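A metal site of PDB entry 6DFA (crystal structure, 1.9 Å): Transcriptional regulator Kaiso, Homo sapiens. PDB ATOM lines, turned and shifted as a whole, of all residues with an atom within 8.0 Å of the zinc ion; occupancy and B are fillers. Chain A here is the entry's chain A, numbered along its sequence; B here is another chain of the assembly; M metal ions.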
ATOM      1  N   ASP A  12      27.391  30.158 -14.708  1.00  0.00           N
ATOM      2  CA  ASP A  12      26.710  28.965 -15.217  1.00  0.00           C
ATOM      3  C   ASP A  12      27.659  27.792 -15.496  1.00  0.00           C
ATOM      4  O   ASP A  12      27.230  26.737 -15.970  1.00  0.00           O
ATOM      5  CB  ASP A  12      25.908  29.295 -16.490  1.00  0.00           C
ATOM      6  CG  ASP A  12      26.779  29.620 -17.683  1.00  0.00           C
ATOM      7  OD1 ASP A  12      26.243  29.642 -18.809  1.00  0.00           O
ATOM      8  OD2 ASP A  12      27.994  29.846 -17.510  1.00  0.00           O
ATOM      9  N   ILE A  25      32.471  23.088 -17.776  1.00  0.00           N
ATOM     10  CA  ILE A  25      31.628  22.142 -17.045  1.00  0.00           C
ATOM     11  C   ILE A  25      30.341  22.813 -16.627  1.00  0.00           C
ATOM     12  O   ILE A  25      30.365  23.828 -15.939  1.00  0.00           O
ATOM     13  CB  ILE A  25      32.341  21.591 -15.784  1.00  0.00           C
ATOM     14  CG1 ILE A  25      33.805  21.259 -16.074  1.00  0.00           C
ATOM     15  CG2 ILE A  25      31.582  20.384 -15.225  1.00  0.00           C
ATOM     16  CD1 ILE A  25      33.998  20.180 -17.116  1.00  0.00           C
ATOM     17  N   CYS A  26      29.213  22.259 -17.048  1.00  0.00           N
ATOM     18  CA  CYS A  26      27.928  22.734 -16.579  1.00  0.00           C
ATOM     19  C   CYS A  26      27.769  22.546 -15.068  1.00  0.00           C
ATOM     20  O   CYS A  26      28.073  21.472 -14.561  1.00  0.00           O
ATOM     21  CB  CYS A  26      26.807  22.012 -17.291  1.00  0.00           C
ATOM     22  SG  CYS A  26      25.229  22.541 -16.712  1.00  0.00           S
ATOM     23  N   ILE A  27      27.264  23.541 -14.336  1.00  0.00           N
ATOM     24  CA  ILE A  27      27.129  23.372 -12.885  1.00  0.00           C
ATOM     25  C   ILE A  27      26.076  22.350 -12.546  1.00  0.00           C
ATOM     26  O   ILE A  27      26.197  21.607 -11.580  1.00  0.00           O
ATOM     27  CB  ILE A  27      26.714  24.629 -12.161  1.00  0.00           C
ATOM     28  CG1 ILE A  27      27.401  25.850 -12.735  1.00  0.00           C
ATOM     29  CG2 ILE A  27      27.038  24.538 -10.655  1.00  0.00           C
ATOM     30  CD1 ILE A  27      26.622  27.053 -12.405  1.00  0.00           C
ATOM     31  N   VAL A  28      25.011  22.352 -13.350  1.00  0.00           N
ATOM     32  CA  VAL A  28      23.824  21.633 -12.948  1.00  0.00           C
ATOM     33  C   VAL A  28      24.026  20.137 -13.143  1.00  0.00           C
ATOM     34  O   VAL A  28      23.896  19.351 -12.200  1.00  0.00           O
ATOM     35  CB  VAL A  28      22.593  22.126 -13.693  1.00  0.00           C
ATOM     36  CG1 VAL A  28      21.382  21.270 -13.362  1.00  0.00           C
ATOM     37  CG2 VAL A  28      22.343  23.590 -13.346  1.00  0.00           C
ATOM     38  N   CYS A  29      24.384  19.738 -14.373  1.00  0.00           N
ATOM     39  CA  CYS A  29      24.527  18.319 -14.669  1.00  0.00           C
ATOM     40  C   CYS A  29      25.981  17.870 -14.796  1.00  0.00           C
ATOM     41  O   CYS A  29      26.248  16.667 -14.894  1.00  0.00           O
ATOM     42  CB  CYS A  29      23.753  17.995 -15.938  1.00  0.00           C
ATOM     43  SG  CYS A  29      24.324  18.890 -17.396  1.00  0.00           S
ATOM     44  N   LYS A  30      26.905  18.819 -14.781  1.00  0.00           N
ATOM     45  CA  LYS A  30      28.348  18.564 -14.900  1.00  0.00           C
ATOM     46  C   LYS A  30      28.779  17.933 -16.235  1.00  0.00           C
ATOM     47  O   LYS A  30      29.800  17.251 -16.306  1.00  0.00           O
ATOM     48  CB  LYS A  30      28.839  17.691 -13.738  1.00  0.00           C
ATOM     49  CG  LYS A  30      28.778  18.400 -12.385  1.00  0.00           C
ATOM     50  CD  LYS A  30      29.551  17.676 -11.305  1.00  0.00           C
ATOM     51  CE  LYS A  30      29.513  18.469 -10.015  1.00  0.00           C
ATOM     52  NZ  LYS A  30      28.115  18.914  -9.722  1.00  0.00           N
ATOM     53  N   ARG A  31      28.015  18.174 -17.305  1.00  0.00           N
ATOM     54  CA  ARG A  31      28.464  17.758 -18.628  1.00  0.00           C
ATOM     55  C   ARG A  31      29.635  18.631 -19.056  1.00  0.00           C
ATOM     56  O   ARG A  31      29.642  19.830 -18.768  1.00  0.00           O
ATOM     57  CB  ARG A  31      27.338  17.848 -19.670  1.00  0.00           C
ATOM     58  CG  ARG A  31      26.345  16.711 -19.579  1.00  0.00           C
ATOM     59  CD  ARG A  31      25.175  16.913 -20.535  1.00  0.00           C
ATOM     60  NE  ARG A  31      24.103  15.968 -20.249  1.00  0.00           N
ATOM     61  CZ  ARG A  31      23.821  14.902 -21.011  1.00  0.00           C
ATOM     62  NH1 ARG A  31      24.530  14.666 -22.110  1.00  0.00           N
ATOM     63  NH2 ARG A  31      22.836  14.091 -20.658  1.00  0.00           N
ATOM     64  N   SER A  32      30.611  18.047 -19.754  1.00  0.00           N
ATOM     65  CA  SER A  32      31.768  18.817 -20.220  1.00  0.00           C
ATOM     66  C   SER A  32      31.658  19.222 -21.678  1.00  0.00           C
ATOM     67  O   SER A  32      31.143  18.486 -22.528  1.00  0.00           O
ATOM     68  CB  SER A  32      33.074  18.039 -19.985  1.00  0.00           C
ATOM     69  OG  SER A  32      33.166  16.915 -20.837  1.00  0.00           O
ATOM     70  N   TYR A  33      32.162  20.424 -21.964  1.00  0.00           N
ATOM     71  CA  TYR A  33      32.121  20.974 -23.305  1.00  0.00           C
ATOM     72  C   TYR A  33      33.481  21.520 -23.670  1.00  0.00           C
ATOM     73  O   TYR A  33      34.186  22.107 -22.840  1.00  0.00           O
ATOM     74  CB  TYR A  33      31.034  22.067 -23.383  1.00  0.00           C
ATOM     75  CG  TYR A  33      29.679  21.465 -23.120  1.00  0.00           C
ATOM     76  CD1 TYR A  33      29.144  21.426 -21.828  1.00  0.00           C
ATOM     77  CD2 TYR A  33      28.956  20.877 -24.154  1.00  0.00           C
ATOM     78  CE1 TYR A  33      27.896  20.848 -21.585  1.00  0.00           C
ATOM     79  CE2 TYR A  33      27.723  20.293 -23.928  1.00  0.00           C
ATOM     80  CZ  TYR A  33      27.196  20.283 -22.646  1.00  0.00           C
ATOM     81  OH  TYR A  33      25.972  19.699 -22.435  1.00  0.00           O
ATOM     82  N   LEU A  39      28.283  24.929 -24.204  1.00  0.00           N
ATOM     83  CA  LEU A  39      27.785  24.958 -22.832  1.00  0.00           C
ATOM     84  C   LEU A  39      26.555  25.874 -22.728  1.00  0.00           C
ATOM     85  O   LEU A  39      25.546  25.489 -22.132  1.00  0.00           O
ATOM     86  CB  LEU A  39      28.900  25.421 -21.871  1.00  0.00           C
ATOM     87  CG  LEU A  39      28.632  25.590 -20.365  1.00  0.00           C
ATOM     88  CD1 LEU A  39      27.957  26.922 -20.031  1.00  0.00           C
ATOM     89  CD2 LEU A  39      27.856  24.425 -19.796  1.00  0.00           C
ATOM     90  N   HIS A  42      23.575  24.391 -24.515  1.00  0.00           N
ATOM     91  CA  HIS A  42      23.082  23.330 -23.661  1.00  0.00           C
ATOM     92  C   HIS A  42      22.329  23.844 -22.434  1.00  0.00           C
ATOM     93  O   HIS A  42      21.318  23.269 -22.009  1.00  0.00           O
ATOM     94  CB  HIS A  42      24.244  22.460 -23.207  1.00  0.00           C
ATOM     95  CG  HIS A  42      23.947  21.729 -21.942  1.00  0.00           C
ATOM     96  ND1 HIS A  42      23.134  20.604 -21.902  1.00  0.00           N
ATOM     97  CD2 HIS A  42      24.333  21.960 -20.667  1.00  0.00           C
ATOM     98  CE1 HIS A  42      23.039  20.183 -20.661  1.00  0.00           C
ATOM     99  NE2 HIS A  42      23.752  20.981 -19.891  1.00  0.00           N
ATOM    100  N   PHE A  43      22.827  24.927 -21.841  1.00  0.00           N
ATOM    101  CA  PHE A  43      22.335  25.362 -20.536  1.00  0.00           C
ATOM    102  C   PHE A  43      20.858  25.797 -20.542  1.00  0.00           C
ATOM    103  O   PHE A  43      20.172  25.730 -19.523  1.00  0.00           O
ATOM    104  CB  PHE A  43      23.202  26.499 -19.999  1.00  0.00           C
ATOM    105  CG  PHE A  43      23.078  26.707 -18.511  1.00  0.00           C
ATOM    106  CD1 PHE A  43      23.806  25.928 -17.622  1.00  0.00           C
ATOM    107  CD2 PHE A  43      22.227  27.674 -17.997  1.00  0.00           C
ATOM    108  CE1 PHE A  43      23.696  26.115 -16.258  1.00  0.00           C
ATOM    109  CE2 PHE A  43      22.106  27.875 -16.620  1.00  0.00           C
ATOM    110  CZ  PHE A  43      22.850  27.090 -15.748  1.00  0.00           C
ATOM    111  N   ASN A  44      20.364  26.227 -21.708  1.00  0.00           N
ATOM    112  CA  ASN A  44      18.974  26.644 -21.816  1.00  0.00           C
ATOM    113  C   ASN A  44      18.013  25.552 -21.370  1.00  0.00           C
ATOM    114  O   ASN A  44      16.914  25.816 -20.894  1.00  0.00           O
ATOM    115  CB  ASN A  44      18.638  27.054 -23.251  1.00  0.00           C
ATOM    116  CG  ASN A  44      17.418  27.948 -23.326  1.00  0.00           C
ATOM    117  OD1 ASN A  44      17.281  28.910 -22.542  1.00  0.00           O
ATOM    118  ND2 ASN A  44      16.484  27.622 -24.220  1.00  0.00           N
ATOM    119  N   ILE A  45      18.447  24.310 -21.557  1.00  0.00           N
ATOM    120  CA  ILE A  45      17.699  23.146 -21.079  1.00  0.00           C
ATOM    121  C   ILE A  45      17.407  23.252 -19.571  1.00  0.00           C
ATOM    122  O   ILE A  45      16.331  22.880 -19.115  1.00  0.00           O
ATOM    123  CB  ILE A  45      18.484  21.854 -21.370  1.00  0.00           C
ATOM    124  CG1 ILE A  45      18.557  21.626 -22.888  1.00  0.00           C
ATOM    125  CG2 ILE A  45      17.853  20.661 -20.672  1.00  0.00           C
ATOM    126  CD1 ILE A  45      19.677  20.699 -23.308  1.00  0.00           C
ATOM    127  N   HIS A  46      18.370  23.777 -18.812  1.00  0.00           N
ATOM    128  CA  HIS A  46      18.176  23.964 -17.377  1.00  0.00           C
ATOM    129  C   HIS A  46      17.406  25.248 -17.057  1.00  0.00           C
ATOM    130  O   HIS A  46      16.519  25.252 -16.208  1.00  0.00           O
ATOM    131  CB  HIS A  46      19.531  24.007 -16.647  1.00  0.00           C
ATOM    132  CG  HIS A  46      20.367  22.785 -16.864  1.00  0.00           C
ATOM    133  ND1 HIS A  46      19.867  21.503 -16.753  1.00  0.00           N
ATOM    134  CD2 HIS A  46      21.681  22.654 -17.185  1.00  0.00           C
ATOM    135  CE1 HIS A  46      20.836  20.636 -16.995  1.00  0.00           C
ATOM    136  NE2 HIS A  46      21.944  21.308 -17.262  1.00  0.00           N
ATOM    137  P    DT B   8      26.010  17.154 -24.982  1.00  0.00           P
ATOM    138  OP1  DT B   8      26.798  16.395 -23.980  1.00  0.00           O
ATOM    139  OP2  DT B   8      25.184  18.301 -24.519  1.00  0.00           O
ATOM    140  O5'  DT B   8      27.014  17.712 -26.084  1.00  0.00           O
ATOM    141  C5'  DT B   8      28.058  16.902 -26.551  1.00  0.00           C
ATOM    142  C4'  DT B   8      28.750  17.513 -27.746  1.00  0.00           C
ATOM    143  O4'  DT B   8      27.869  17.479 -28.917  1.00  0.00           O
ATOM    144  C3'  DT B   8      29.155  18.978 -27.595  1.00  0.00           C
ATOM    145  O3'  DT B   8      30.380  19.139 -28.275  1.00  0.00           O
ATOM    146  C2'  DT B   8      28.020  19.712 -28.357  1.00  0.00           C
ATOM    147  C1'  DT B   8      27.863  18.742 -29.510  1.00  0.00           C
ATOM    148  N1   DT B   8      26.619  18.868 -30.326  1.00  0.00           N
ATOM    149  C2   DT B   8      26.642  18.324 -31.585  1.00  0.00           C
ATOM    150  O2   DT B   8      27.634  17.794 -32.055  1.00  0.00           O
ATOM    151  N3   DT B   8      25.474  18.457 -32.292  1.00  0.00           N
ATOM    152  C4   DT B   8      24.294  19.027 -31.857  1.00  0.00           C
ATOM    153  O4   DT B   8      23.294  19.080 -32.579  1.00  0.00           O
ATOM    154  C5   DT B   8      24.330  19.570 -30.524  1.00  0.00           C
ATOM    155  C7   DT B   8      23.108  20.236 -29.957  1.00  0.00           C
ATOM    156  C6   DT B   8      25.481  19.463 -29.815  1.00  0.00           C
HETATM  157 ZN    ZN M   1      23.838  20.974 -17.792  1.00  0.00          ZN
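The side-chain hydroxyl of Tyr 33 sits close to a ring nitrogen (ND1) of His 42, at 3.0 Å.
N of Arg 31 lies close to SG of Cys 29.
The side-chain sulfur (SG) of Cys 26 lies close to the backbone NH (N) of Val 28 (3.4 Å).
O of Arg 31 lies within hydrogen-bond range of N of Cys 26, at 3.0 Å.
Of the 17 residues printed, 4 come within 4 Å of the zinc ion.
The nearest printed residue that does not touch the zinc ion is Val 28 (4.4 Å).
The zinc ion is bound by NE2 of His 46 (2.0 Å), NE2 of His 42 (2.1 Å), SG of Cys 29 (2.2 Å) and SG of Cys 26 (2.4 Å).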
